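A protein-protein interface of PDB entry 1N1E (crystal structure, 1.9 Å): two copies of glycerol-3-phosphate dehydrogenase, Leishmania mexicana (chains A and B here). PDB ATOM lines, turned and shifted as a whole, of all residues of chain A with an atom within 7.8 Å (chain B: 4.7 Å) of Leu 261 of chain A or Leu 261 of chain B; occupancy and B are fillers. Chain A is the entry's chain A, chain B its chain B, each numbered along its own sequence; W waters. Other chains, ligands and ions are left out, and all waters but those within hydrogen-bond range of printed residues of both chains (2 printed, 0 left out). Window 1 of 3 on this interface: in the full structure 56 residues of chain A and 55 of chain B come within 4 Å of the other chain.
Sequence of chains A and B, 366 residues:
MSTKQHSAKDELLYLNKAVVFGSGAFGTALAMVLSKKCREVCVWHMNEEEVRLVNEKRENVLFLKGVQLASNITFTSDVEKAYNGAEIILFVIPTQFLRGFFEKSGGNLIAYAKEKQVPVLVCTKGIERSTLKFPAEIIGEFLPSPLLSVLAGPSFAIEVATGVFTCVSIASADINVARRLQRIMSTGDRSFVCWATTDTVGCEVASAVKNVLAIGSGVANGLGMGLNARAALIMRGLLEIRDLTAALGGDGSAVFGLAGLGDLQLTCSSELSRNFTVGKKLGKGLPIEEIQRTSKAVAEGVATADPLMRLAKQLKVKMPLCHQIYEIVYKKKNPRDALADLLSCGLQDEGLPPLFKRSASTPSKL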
ATOM      1  N   PRO A 154      20.341 -10.964 -31.812  1.00  0.00           N
ATOM      2  CA  PRO A 154      21.568 -10.673 -31.074  1.00  0.00           C
ATOM      3  C   PRO A 154      22.468 -11.897 -31.077  1.00  0.00           C
ATOM      4  O   PRO A 154      22.261 -12.826 -30.303  1.00  0.00           O
ATOM      5  CB  PRO A 154      21.069 -10.337 -29.673  1.00  0.00           C
ATOM      6  CG  PRO A 154      19.731 -10.976 -29.547  1.00  0.00           C
ATOM      7  CD  PRO A 154      19.188 -11.202 -30.923  1.00  0.00           C
ATOM      8  N   ALA A 206      15.587  -3.426 -39.031  1.00  0.00           N
ATOM      9  CA  ALA A 206      16.216  -3.377 -37.722  1.00  0.00           C
ATOM     10  C   ALA A 206      17.685  -3.741 -37.811  1.00  0.00           C
ATOM     11  O   ALA A 206      18.529  -3.046 -37.251  1.00  0.00           O
ATOM     12  CB  ALA A 206      15.483  -4.295 -36.745  1.00  0.00           C
ATOM     13  N   LYS A 210      20.337  -0.835 -36.836  1.00  0.00           N
ATOM     14  CA  LYS A 210      20.990  -1.013 -35.536  1.00  0.00           C
ATOM     15  C   LYS A 210      22.491  -0.825 -35.673  1.00  0.00           C
ATOM     16  O   LYS A 210      23.138  -0.346 -34.750  1.00  0.00           O
ATOM     17  CB  LYS A 210      20.658  -2.362 -34.880  1.00  0.00           C
ATOM     18  CG  LYS A 210      21.168  -3.599 -35.622  1.00  0.00           C
ATOM     19  CD  LYS A 210      22.524  -4.073 -35.092  1.00  0.00           C
ATOM     20  CE  LYS A 210      23.095  -5.203 -35.926  1.00  0.00           C
ATOM     21  NZ  LYS A 210      24.327  -5.758 -35.319  1.00  0.00           N
ATOM     22  N   ALA A 231      21.676   3.888 -22.534  1.00  0.00           N
ATOM     23  CA  ALA A 231      20.327   3.342 -22.421  1.00  0.00           C
ATOM     24  C   ALA A 231      19.334   4.260 -23.125  1.00  0.00           C
ATOM     25  O   ALA A 231      18.415   3.807 -23.798  1.00  0.00           O
ATOM     26  CB  ALA A 231      19.956   3.176 -20.968  1.00  0.00           C
ATOM     27  N   ALA A 232      19.549   5.560 -22.984  1.00  0.00           N
ATOM     28  CA  ALA A 232      18.701   6.548 -23.625  1.00  0.00           C
ATOM     29  C   ALA A 232      18.849   6.502 -25.151  1.00  0.00           C
ATOM     30  O   ALA A 232      17.854   6.609 -25.861  1.00  0.00           O
ATOM     31  CB  ALA A 232      19.027   7.926 -23.100  1.00  0.00           C
ATOM     32  N   LEU A 233      20.078   6.344 -25.646  1.00  0.00           N
ATOM     33  CA  LEU A 233      20.334   6.198 -27.077  1.00  0.00           C
ATOM     34  C   LEU A 233      19.651   4.954 -27.637  1.00  0.00           C
ATOM     35  O   LEU A 233      19.067   5.005 -28.705  1.00  0.00           O
ATOM     36  CB  LEU A 233      21.837   6.151 -27.367  1.00  0.00           C
ATOM     37  CG  LEU A 233      22.194   5.955 -28.848  1.00  0.00           C
ATOM     38  CD1 LEU A 233      23.351   6.843 -29.258  1.00  0.00           C
ATOM     39  CD2 LEU A 233      22.511   4.503 -29.162  1.00  0.00           C
ATOM     40  N   ILE A 234      19.717   3.841 -26.912  1.00  0.00           N
ATOM     41  CA  ILE A 234      19.077   2.604 -27.355  1.00  0.00           C
ATOM     42  C   ILE A 234      17.560   2.791 -27.439  1.00  0.00           C
ATOM     43  O   ILE A 234      16.924   2.405 -28.427  1.00  0.00           O
ATOM     44  CB  ILE A 234      19.435   1.432 -26.404  1.00  0.00           C
ATOM     45  CG1 ILE A 234      20.900   1.034 -26.586  1.00  0.00           C
ATOM     46  CG2 ILE A 234      18.545   0.231 -26.669  1.00  0.00           C
ATOM     47  CD1 ILE A 234      21.499   0.251 -25.388  1.00  0.00           C
ATOM     48  N   MET A 235      16.993   3.408 -26.407  1.00  0.00           N
ATOM     49  CA  MET A 235      15.556   3.612 -26.330  1.00  0.00           C
ATOM     50  C   MET A 235      15.056   4.553 -27.444  1.00  0.00           C
ATOM     51  O   MET A 235      14.094   4.232 -28.158  1.00  0.00           O
ATOM     52  CB  MET A 235      15.191   4.131 -24.938  1.00  0.00           C
ATOM     53  CG  MET A 235      13.714   4.238 -24.676  1.00  0.00           C
ATOM     54  SD  MET A 235      13.109   5.884 -24.955  1.00  0.00           S
ATOM     55  CE  MET A 235      11.884   5.603 -26.204  1.00  0.00           C
ATOM     56  N   ARG A 236      15.719   5.691 -27.615  1.00  0.00           N
ATOM     57  CA  ARG A 236      15.329   6.642 -28.654  1.00  0.00           C
ATOM     58  C   ARG A 236      15.609   6.089 -30.052  1.00  0.00           C
ATOM     59  O   ARG A 236      14.831   6.305 -30.982  1.00  0.00           O
ATOM     60  CB  ARG A 236      16.023   7.997 -28.460  1.00  0.00           C
ATOM     61  CG  ARG A 236      15.689   8.745 -27.158  1.00  0.00           C
ATOM     62  CD  ARG A 236      14.215   8.938 -26.814  1.00  0.00           C
ATOM     63  NE  ARG A 236      13.501   9.785 -27.759  1.00  0.00           N
ATOM     64  CZ  ARG A 236      12.202  10.080 -27.672  1.00  0.00           C
ATOM     65  NH1 ARG A 236      11.462   9.617 -26.669  1.00  0.00           N
ATOM     66  NH2 ARG A 236      11.635  10.846 -28.598  1.00  0.00           N
ATOM     67  N   LEU A 238      15.512   3.037 -31.136  1.00  0.00           N
ATOM     68  CA  LEU A 238      14.555   2.025 -31.532  1.00  0.00           C
ATOM     69  C   LEU A 238      13.326   2.669 -32.174  1.00  0.00           C
ATOM     70  O   LEU A 238      12.694   2.064 -33.024  1.00  0.00           O
ATOM     71  CB  LEU A 238      14.154   1.156 -30.343  1.00  0.00           C
ATOM     72  CG  LEU A 238      13.643  -0.269 -30.605  1.00  0.00           C
ATOM     73  CD1 LEU A 238      14.454  -1.051 -31.634  1.00  0.00           C
ATOM     74  CD2 LEU A 238      13.637  -1.023 -29.282  1.00  0.00           C
ATOM     75  N   LEU A 239      13.019   3.901 -31.794  1.00  0.00           N
ATOM     76  CA  LEU A 239      11.918   4.637 -32.416  1.00  0.00           C
ATOM     77  C   LEU A 239      12.171   4.905 -33.881  1.00  0.00           C
ATOM     78  O   LEU A 239      11.228   4.987 -34.659  1.00  0.00           O
ATOM     79  CB  LEU A 239      11.672   5.972 -31.717  1.00  0.00           C
ATOM     80  CG  LEU A 239      11.450   5.923 -30.210  1.00  0.00           C
ATOM     81  CD1 LEU A 239      11.318   7.339 -29.670  1.00  0.00           C
ATOM     82  CD2 LEU A 239      10.236   5.092 -29.875  1.00  0.00           C
ATOM     83  N   ILE A 241      14.073   2.896 -35.879  1.00  0.00           N
ATOM     84  CA  ILE A 241      13.818   1.592 -36.478  1.00  0.00           C
ATOM     85  C   ILE A 241      12.321   1.387 -36.687  1.00  0.00           C
ATOM     86  O   ILE A 241      11.905   0.946 -37.745  1.00  0.00           O
ATOM     87  CB  ILE A 241      14.371   0.446 -35.585  1.00  0.00           C
ATOM     88  CG1 ILE A 241      15.900   0.428 -35.661  1.00  0.00           C
ATOM     89  CG2 ILE A 241      13.774  -0.903 -36.003  1.00  0.00           C
ATOM     90  CD1 ILE A 241      16.567  -0.574 -34.714  1.00  0.00           C
ATOM     91  N   ALA A 254       8.779  -7.323 -35.290  1.00  0.00           N
ATOM     92  CA  ALA A 254      10.204  -7.560 -35.067  1.00  0.00           C
ATOM     93  C   ALA A 254      10.901  -6.414 -34.331  1.00  0.00           C
ATOM     94  O   ALA A 254      11.987  -6.614 -33.791  1.00  0.00           O
ATOM     95  CB  ALA A 254      10.909  -7.839 -36.385  1.00  0.00           C
ATOM     96  N   VAL A 255      10.288  -5.228 -34.301  1.00  0.00           N
ATOM     97  CA  VAL A 255      10.945  -4.037 -33.746  1.00  0.00           C
ATOM     98  C   VAL A 255      11.362  -4.228 -32.279  1.00  0.00           C
ATOM     99  O   VAL A 255      12.480  -3.884 -31.900  1.00  0.00           O
ATOM    100  CB  VAL A 255      10.052  -2.773 -33.849  1.00  0.00           C
ATOM    101  CG1 VAL A 255      10.669  -1.611 -33.071  1.00  0.00           C
ATOM    102  CG2 VAL A 255       9.842  -2.373 -35.313  1.00  0.00           C
ATOM    103  N   PHE A 256      10.454  -4.762 -31.468  1.00  0.00           N
ATOM    104  CA  PHE A 256      10.728  -5.024 -30.058  1.00  0.00           C
ATOM    105  C   PHE A 256      11.021  -6.517 -29.804  1.00  0.00           C
ATOM    106  O   PHE A 256      10.955  -6.996 -28.676  1.00  0.00           O
ATOM    107  CB  PHE A 256       9.571  -4.498 -29.207  1.00  0.00           C
ATOM    108  CG  PHE A 256       9.371  -3.006 -29.346  1.00  0.00           C
ATOM    109  CD1 PHE A 256       8.240  -2.494 -29.959  1.00  0.00           C
ATOM    110  CD2 PHE A 256      10.356  -2.126 -28.916  1.00  0.00           C
ATOM    111  CE1 PHE A 256       8.069  -1.116 -30.104  1.00  0.00           C
ATOM    112  CE2 PHE A 256      10.199  -0.740 -29.064  1.00  0.00           C
ATOM    113  CZ  PHE A 256       9.056  -0.240 -29.662  1.00  0.00           C
ATOM    114  N   GLY A 257      11.369  -7.225 -30.874  1.00  0.00           N
ATOM    115  CA  GLY A 257      11.767  -8.614 -30.818  1.00  0.00           C
ATOM    116  C   GLY A 257      13.264  -8.730 -30.942  1.00  0.00           C
ATOM    117  O   GLY A 257      13.994  -7.772 -30.746  1.00  0.00           O
ATOM    118  N   LEU A 258      13.734  -9.924 -31.277  1.00  0.00           N
ATOM    119  CA  LEU A 258      15.162 -10.202 -31.273  1.00  0.00           C
ATOM    120  C   LEU A 258      15.933  -9.381 -32.312  1.00  0.00           C
ATOM    121  O   LEU A 258      17.038  -8.924 -32.038  1.00  0.00           O
ATOM    122  CB  LEU A 258      15.407 -11.701 -31.463  1.00  0.00           C
ATOM    123  CG  LEU A 258      14.962 -12.594 -30.290  1.00  0.00           C
ATOM    124  CD1 LEU A 258      14.902 -14.062 -30.723  1.00  0.00           C
ATOM    125  CD2 LEU A 258      15.913 -12.405 -29.094  1.00  0.00           C
ATOM    126  N   ALA A 259      15.340  -9.179 -33.484  1.00  0.00           N
ATOM    127  CA  ALA A 259      15.987  -8.461 -34.579  1.00  0.00           C
ATOM    128  C   ALA A 259      16.172  -6.982 -34.279  1.00  0.00           C
ATOM    129  O   ALA A 259      17.178  -6.380 -34.677  1.00  0.00           O
ATOM    130  CB  ALA A 259      15.194  -8.620 -35.859  1.00  0.00           C
ATOM    131  N   GLY A 260      15.208  -6.402 -33.577  1.00  0.00           N
ATOM    132  CA  GLY A 260      15.264  -4.995 -33.248  1.00  0.00           C
ATOM    133  C   GLY A 260      15.867  -4.760 -31.886  1.00  0.00           C
ATOM    134  O   GLY A 260      17.075  -4.632 -31.750  1.00  0.00           O
ATOM    135  N   LEU A 261      15.013  -4.703 -30.875  1.00  0.00           N
ATOM    136  CA  LEU A 261      15.431  -4.465 -29.505  1.00  0.00           C
ATOM    137  C   LEU A 261      16.626  -5.328 -29.088  1.00  0.00           C
ATOM    138  O   LEU A 261      17.592  -4.828 -28.541  1.00  0.00           O
ATOM    139  CB  LEU A 261      14.236  -4.746 -28.591  1.00  0.00           C
ATOM    140  CG  LEU A 261      14.338  -4.530 -27.080  1.00  0.00           C
ATOM    141  CD1 LEU A 261      12.953  -4.236 -26.531  1.00  0.00           C
ATOM    142  CD2 LEU A 261      14.889  -5.711 -26.362  1.00  0.00           C
ATOM    143  N   GLY A 262      16.557  -6.623 -29.364  1.00  0.00           N
ATOM    144  CA  GLY A 262      17.586  -7.555 -28.930  1.00  0.00           C
ATOM    145  C   GLY A 262      18.944  -7.241 -29.521  1.00  0.00           C
ATOM    146  O   GLY A 262      19.924  -7.056 -28.805  1.00  0.00           O
ATOM    147  N   ASP A 263      18.987  -7.163 -30.843  1.00  0.00           N
ATOM    148  CA  ASP A 263      20.226  -6.971 -31.568  1.00  0.00           C
ATOM    149  C   ASP A 263      20.778  -5.547 -31.344  1.00  0.00           C
ATOM    150  O   ASP A 263      21.984  -5.344 -31.235  1.00  0.00           O
ATOM    151  CB  ASP A 263      19.973  -7.259 -33.056  1.00  0.00           C
ATOM    152  CG  ASP A 263      21.241  -7.449 -33.845  1.00  0.00           C
ATOM    153  OD1 ASP A 263      21.140  -7.623 -35.083  1.00  0.00           O
ATOM    154  OD2 ASP A 263      22.374  -7.439 -33.340  1.00  0.00           O
ATOM    155  N   LEU A 264      19.887  -4.565 -31.267  1.00  0.00           N
ATOM    156  CA  LEU A 264      20.299  -3.183 -31.026  1.00  0.00           C
ATOM    157  C   LEU A 264      20.959  -3.063 -29.661  1.00  0.00           C
ATOM    158  O   LEU A 264      22.048  -2.514 -29.522  1.00  0.00           O
ATOM    159  CB  LEU A 264      19.091  -2.251 -31.072  1.00  0.00           C
ATOM    160  CG  LEU A 264      19.333  -0.779 -30.759  1.00  0.00           C
ATOM    161  CD1 LEU A 264      20.212  -0.147 -31.820  1.00  0.00           C
ATOM    162  CD2 LEU A 264      18.039  -0.034 -30.637  1.00  0.00           C
ATOM    163  N   GLN A 265      20.279  -3.572 -28.644  1.00  0.00           N
ATOM    164  CA  GLN A 265      20.796  -3.453 -27.295  1.00  0.00           C
ATOM    165  C   GLN A 265      22.143  -4.165 -27.177  1.00  0.00           C
ATOM    166  O   GLN A 265      23.051  -3.664 -26.529  1.00  0.00           O
ATOM    167  CB  GLN A 265      19.754  -3.926 -26.264  1.00  0.00           C
ATOM    168  CG  GLN A 265      19.861  -5.341 -25.873  1.00  0.00           C
ATOM    169  CD  GLN A 265      21.002  -5.574 -24.941  1.00  0.00           C
ATOM    170  OE1 GLN A 265      21.294  -4.731 -24.116  1.00  0.00           O
ATOM    171  NE2 GLN A 265      21.669  -6.696 -25.085  1.00  0.00           N
ATOM    172  N   LEU A 266      22.302  -5.290 -27.867  1.00  0.00           N
ATOM    173  CA  LEU A 266      23.546  -6.051 -27.822  1.00  0.00           C
ATOM    174  C   LEU A 266      24.708  -5.273 -28.440  1.00  0.00           C
ATOM    175  O   LEU A 266      25.764  -5.115 -27.838  1.00  0.00           O
ATOM    176  CB  LEU A 266      23.373  -7.380 -28.571  1.00  0.00           C
ATOM    177  CG  LEU A 266      24.641  -8.212 -28.824  1.00  0.00           C
ATOM    178  CD1 LEU A 266      25.073  -8.947 -27.564  1.00  0.00           C
ATOM    179  CD2 LEU A 266      24.443  -9.201 -29.948  1.00  0.00           C
ATOM    180  N   THR A 267      24.477  -4.808 -29.658  1.00  0.00           N
ATOM    181  CA  THR A 267      25.489  -4.170 -30.495  1.00  0.00           C
ATOM    182  C   THR A 267      25.902  -2.817 -29.951  1.00  0.00           C
ATOM    183  O   THR A 267      27.045  -2.397 -30.122  1.00  0.00           O
ATOM    184  CB  THR A 267      24.922  -4.016 -31.944  1.00  0.00           C
ATOM    185  OG1 THR A 267      24.456  -5.290 -32.418  1.00  0.00           O
ATOM    186  CG2 THR A 267      25.991  -3.686 -32.902  1.00  0.00           C
ATOM    187  N   LEU A 352       5.455   8.166 -26.649  1.00  0.00           N
ATOM    188  CA  LEU A 352       5.185   6.851 -27.215  1.00  0.00           C
ATOM    189  C   LEU A 352       3.677   6.603 -27.190  1.00  0.00           C
ATOM    190  O   LEU A 352       3.006   6.979 -26.227  1.00  0.00           O
ATOM    191  CB  LEU A 352       5.907   5.750 -26.433  1.00  0.00           C
ATOM    192  CG  LEU A 352       7.299   5.377 -26.941  1.00  0.00           C
ATOM    193  CD1 LEU A 352       8.174   6.600 -27.076  1.00  0.00           C
ATOM    194  CD2 LEU A 352       7.952   4.351 -26.010  1.00  0.00           C
ATOM    195  N   ILE B 234      16.663  -9.781 -21.935  1.00  0.00           N
ATOM    196  CA  ILE B 234      16.070  -8.445 -21.926  1.00  0.00           C
ATOM    197  C   ILE B 234      14.843  -8.417 -22.828  1.00  0.00           C
ATOM    198  O   ILE B 234      13.783  -7.935 -22.446  1.00  0.00           O
ATOM    199  CB  ILE B 234      17.104  -7.400 -22.367  1.00  0.00           C
ATOM    200  CG1 ILE B 234      18.196  -7.278 -21.289  1.00  0.00           C
ATOM    201  CG2 ILE B 234      16.426  -6.060 -22.641  1.00  0.00           C
ATOM    202  CD1 ILE B 234      19.471  -6.624 -21.771  1.00  0.00           C
ATOM    203  N   MET B 235      14.986  -8.980 -24.020  1.00  0.00           N
ATOM    204  CA  MET B 235      13.919  -8.935 -25.008  1.00  0.00           C
ATOM    205  C   MET B 235      12.697  -9.742 -24.527  1.00  0.00           C
ATOM    206  O   MET B 235      11.572  -9.255 -24.562  1.00  0.00           O
ATOM    207  CB  MET B 235      14.459  -9.431 -26.360  1.00  0.00           C
ATOM    208  CG  MET B 235      13.477  -9.336 -27.514  1.00  0.00           C
ATOM    209  SD  MET B 235      12.614 -10.927 -27.719  1.00  0.00           S
ATOM    210  CE  MET B 235      10.942 -10.434 -27.524  1.00  0.00           C
ATOM    211  N   LEU B 238      10.951  -8.107 -21.322  1.00  0.00           N
ATOM    212  CA  LEU B 238      10.102  -6.950 -21.578  1.00  0.00           C
ATOM    213  C   LEU B 238       8.656  -7.352 -21.860  1.00  0.00           C
ATOM    214  O   LEU B 238       7.727  -6.601 -21.559  1.00  0.00           O
ATOM    215  CB  LEU B 238      10.635  -6.125 -22.756  1.00  0.00           C
ATOM    216  CG  LEU B 238      10.083  -4.714 -22.894  1.00  0.00           C
ATOM    217  CD1 LEU B 238      10.234  -3.898 -21.609  1.00  0.00           C
ATOM    218  CD2 LEU B 238      10.807  -4.016 -24.031  1.00  0.00           C
ATOM    219  N   ALA B 254       4.811   3.446 -21.452  1.00  0.00           N
ATOM    220  CA  ALA B 254       6.083   3.391 -20.740  1.00  0.00           C
ATOM    221  C   ALA B 254       6.912   2.157 -21.090  1.00  0.00           C
ATOM    222  O   ALA B 254       8.140   2.163 -20.919  1.00  0.00           O
ATOM    223  CB  ALA B 254       5.841   3.435 -19.222  1.00  0.00           C
ATOM    224  N   VAL B 255       6.249   1.102 -21.569  1.00  0.00           N
ATOM    225  CA  VAL B 255       6.896  -0.203 -21.762  1.00  0.00           C
ATOM    226  C   VAL B 255       8.138  -0.125 -22.651  1.00  0.00           C
ATOM    227  O   VAL B 255       9.188  -0.703 -22.323  1.00  0.00           O
ATOM    228  CB  VAL B 255       5.905  -1.246 -22.343  1.00  0.00           C
ATOM    229  CG1 VAL B 255       6.623  -2.533 -22.764  1.00  0.00           C
ATOM    230  CG2 VAL B 255       4.820  -1.564 -21.317  1.00  0.00           C
ATOM    231  N   PHE B 256       8.016   0.567 -23.775  1.00  0.00           N
ATOM    232  CA  PHE B 256       9.135   0.685 -24.704  1.00  0.00           C
ATOM    233  C   PHE B 256       9.849   2.042 -24.560  1.00  0.00           C
ATOM    234  O   PHE B 256      10.616   2.440 -25.429  1.00  0.00           O
ATOM    235  CB  PHE B 256       8.650   0.429 -26.134  1.00  0.00           C
ATOM    236  CG  PHE B 256       8.001  -0.935 -26.314  1.00  0.00           C
ATOM    237  CD1 PHE B 256       6.738  -1.056 -26.870  1.00  0.00           C
ATOM    238  CD2 PHE B 256       8.658  -2.085 -25.908  1.00  0.00           C
ATOM    239  CE1 PHE B 256       6.141  -2.305 -27.030  1.00  0.00           C
ATOM    240  CE2 PHE B 256       8.063  -3.340 -26.057  1.00  0.00           C
ATOM    241  CZ  PHE B 256       6.797  -3.440 -26.615  1.00  0.00           C
ATOM    242  N   GLY B 257       9.604   2.723 -23.441  1.00  0.00           N
ATOM    243  CA  GLY B 257      10.233   3.998 -23.140  1.00  0.00           C
ATOM    244  C   GLY B 257      11.321   3.843 -22.100  1.00  0.00           C
ATOM    245  O   GLY B 257      11.855   2.750 -21.894  1.00  0.00           O
ATOM    246  N   LEU B 258      11.627   4.945 -21.424  1.00  0.00           N
ATOM    247  CA  LEU B 258      12.740   5.003 -20.491  1.00  0.00           C
ATOM    248  C   LEU B 258      12.494   4.117 -19.273  1.00  0.00           C
ATOM    249  O   LEU B 258      13.400   3.408 -18.827  1.00  0.00           O
ATOM    250  CB  LEU B 258      13.022   6.463 -20.087  1.00  0.00           C
ATOM    251  CG  LEU B 258      13.607   7.351 -21.197  1.00  0.00           C
ATOM    252  CD1 LEU B 258      13.524   8.820 -20.818  1.00  0.00           C
ATOM    253  CD2 LEU B 258      15.047   6.968 -21.511  1.00  0.00           C
ATOM    254  N   ALA B 259      11.264   4.111 -18.763  1.00  0.00           N
ATOM    255  CA  ALA B 259      10.932   3.347 -17.550  1.00  0.00           C
ATOM    256  C   ALA B 259      11.018   1.828 -17.747  1.00  0.00           C
ATOM    257  O   ALA B 259      11.448   1.073 -16.848  1.00  0.00           O
ATOM    258  CB  ALA B 259       9.531   3.721 -17.061  1.00  0.00           C
ATOM    259  N   GLY B 260      10.599   1.387 -18.921  1.00  0.00           N
ATOM    260  CA  GLY B 260      10.588  -0.022 -19.255  1.00  0.00           C
ATOM    261  C   GLY B 260      11.864  -0.444 -19.933  1.00  0.00           C
ATOM    262  O   GLY B 260      12.833  -0.805 -19.283  1.00  0.00           O
ATOM    263  N   LEU B 261      11.852  -0.400 -21.254  1.00  0.00           N
ATOM    264  CA  LEU B 261      12.979  -0.814 -22.057  1.00  0.00           C
ATOM    265  C   LEU B 261      14.316  -0.188 -21.603  1.00  0.00           C
ATOM    266  O   LEU B 261      15.312  -0.887 -21.441  1.00  0.00           O
ATOM    267  CB  LEU B 261      12.676  -0.469 -23.511  1.00  0.00           C
ATOM    268  CG  LEU B 261      13.553  -1.060 -24.605  1.00  0.00           C
ATOM    269  CD1 LEU B 261      12.740  -1.118 -25.891  1.00  0.00           C
ATOM    270  CD2 LEU B 261      14.792  -0.241 -24.810  1.00  0.00           C
ATOM    271  N   GLY B 262      14.339   1.116 -21.373  1.00  0.00           N
ATOM    272  CA  GLY B 262      15.589   1.796 -21.060  1.00  0.00           C
ATOM    273  C   GLY B 262      16.208   1.299 -19.759  1.00  0.00           C
ATOM    274  O   GLY B 262      17.382   0.910 -19.713  1.00  0.00           O
ATOM    275  N   ASP B 263      15.400   1.290 -18.708  1.00  0.00           N
ATOM    276  CA  ASP B 263      15.844   0.894 -17.371  1.00  0.00           C
ATOM    277  C   ASP B 263      16.126  -0.612 -17.311  1.00  0.00           C
ATOM    278  O   ASP B 263      17.088  -1.043 -16.685  1.00  0.00           O
ATOM    279  CB  ASP B 263      14.779   1.283 -16.345  1.00  0.00           C
ATOM    280  CG  ASP B 263      15.292   1.289 -14.925  1.00  0.00           C
ATOM    281  OD1 ASP B 263      14.466   1.534 -14.010  1.00  0.00           O
ATOM    282  OD2 ASP B 263      16.477   1.063 -14.611  1.00  0.00           O
ATOM    283  N   LEU B 264      15.285  -1.407 -17.964  1.00  0.00           N
ATOM    284  CA  LEU B 264      15.488  -2.857 -18.024  1.00  0.00           C
ATOM    285  C   LEU B 264      16.838  -3.177 -18.666  1.00  0.00           C
ATOM    286  O   LEU B 264      17.646  -3.903 -18.099  1.00  0.00           O
ATOM    287  CB  LEU B 264      14.355  -3.546 -18.800  1.00  0.00           C
ATOM    288  CG  LEU B 264      14.522  -5.061 -18.983  1.00  0.00           C
ATOM    289  CD1 LEU B 264      14.465  -5.766 -17.621  1.00  0.00           C
ATOM    290  CD2 LEU B 264      13.496  -5.613 -19.938  1.00  0.00           C
ATOM    291  N   GLN B 265      17.099  -2.613 -19.836  1.00  0.00           N
ATOM    292  CA  GLN B 265      18.336  -2.926 -20.533  1.00  0.00           C
ATOM    293  C   GLN B 265      19.575  -2.451 -19.739  1.00  0.00           C
ATOM    294  O   GLN B 265      20.570  -3.173 -19.648  1.00  0.00           O
ATOM    295  CB  GLN B 265      18.305  -2.437 -21.990  1.00  0.00           C
ATOM    296  CG  GLN B 265      18.744  -1.037 -22.210  1.00  0.00           C
ATOM    297  CD  GLN B 265      20.236  -0.872 -22.164  1.00  0.00           C
ATOM    298  OE1 GLN B 265      20.974  -1.706 -22.666  1.00  0.00           O
ATOM    299  NE2 GLN B 265      20.683   0.196 -21.551  1.00  0.00           N
HETATM  300  O   HOH W   1      10.156  -7.186 -26.191  1.00  0.00           O
HETATM  301  O   HOH W   2      11.992   2.249 -27.781  1.00  0.00           O
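Of chain B, only Met 235 (3.6 Å), Leu 238 (3.3 Å) and Leu 261 (3.2 Å) come within 4 Å of Leu 261 of chain A.
Gly 262 of chain A touches none of the printed residues of chain B.
Of the printed residues of chain A, Leu 238 of chain B touches Leu 261 (3.3 Å).
Of the printed residues of chain A, Leu 261 of chain B touches Leu 238, Phe 256 and Leu 261.
Gly 262 of chain B touches just one residue of chain A: Ala 231 (3.7 Å).
The nearest residue of chain B that does not touch Leu 261 of chain A is Ile 234 of chain B (4.04 Å).
The nearest printed residue of chain A that does not touch Leu 261 of chain B is Met 235 of chain A (4.2 Å).
Met 235 of chain A touches Leu 258 of chain B, and with the chains exchanged Leu 258 of chain A touches Met 235 of chain B.
Phe 256 of chain A touches Leu 261 of chain B, but with the chains exchanged Leu 261 of chain A does not touch Phe 256 of chain B (4.8 Å).
The side-chain amide oxygen (OE1) of Gln 265 of chain A lies close to the side-chain amide oxygen (OE1) of Gln 265 of chain B, 3.4 Å away.
Water W1 bridges O of Phe 256 of chain A (2.6 Å) and O of Met 235 of chain B (3.0 Å).
Water W2 bridges the backbone carbonyl oxygen (O) of Phe 256 of chain B (2.7 Å) and the backbone carbonyl oxygen (O) of Met 235 of chain A (2.9 Å).
Among the printed residues, pairs that only touch across the chains: Ala 231 of chain A with Gly 262 of chain B (3.7 Å), Ala 231 of chain A with Gln 265 of chain B (3.1 Å), Ile 234 of chain A with Gln 265 of chain B (3.4 Å), Met 235 of chain A with Phe 256 of chain B (3.5 Å), Met 235 of chain A with Gly 257 of chain B (3.5 Å), Met 235 of chain A with Leu 258 of chain B (3.9 Å), Leu 238 of chain A with Leu 261 of chain B (3.5 Å), Phe 256 of chain A with Met 235 of chain B (3.6 Å), Phe 256 of chain A with Phe 256 of chain B (3.5 Å), Phe 256 of chain A with Leu 261 of chain B (3.98 Å), Gly 257 of chain A with Met 235 of chain B (3.5 Å), Leu 258 of chain A with Met 235 of chain B (3.8 Å), Leu 261 of chain A with Met 235 of chain B (3.6 Å), Leu 261 of chain A with Leu 238 of chain B (3.3 Å), Leu 261 of chain A with Leu 261 of chain B (3.2 Å), Gln 265 of chain A with Ile 234 of chain B (3.5 Å), Leu 352 of chain A with Phe 256 of chain B (3.3 Å) and Leu 352 of chain A with Gly 257 of chain B (3.5 Å).
Of the 15 printed residues of chain B, 9 touch a printed residue of chain A.
Printed residues of chain A that touch a printed residue of chain B: Ala 231, Ile 234, Met 235, Leu 238, Phe 256, Gly 257, Leu 258, Leu 261, Gln 265 and Leu 352.
Among the printed residues, no Asp or Glu carboxylate lies within 4 Å of a Lys or Arg side-chain nitrogen of the other chain.
The backbone carbonyl oxygen (O) of Gly 257 of chain B sits at hydrogen-bond distance from the backbone NH (N) of Gly 262 of chain B (3.0 Å).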
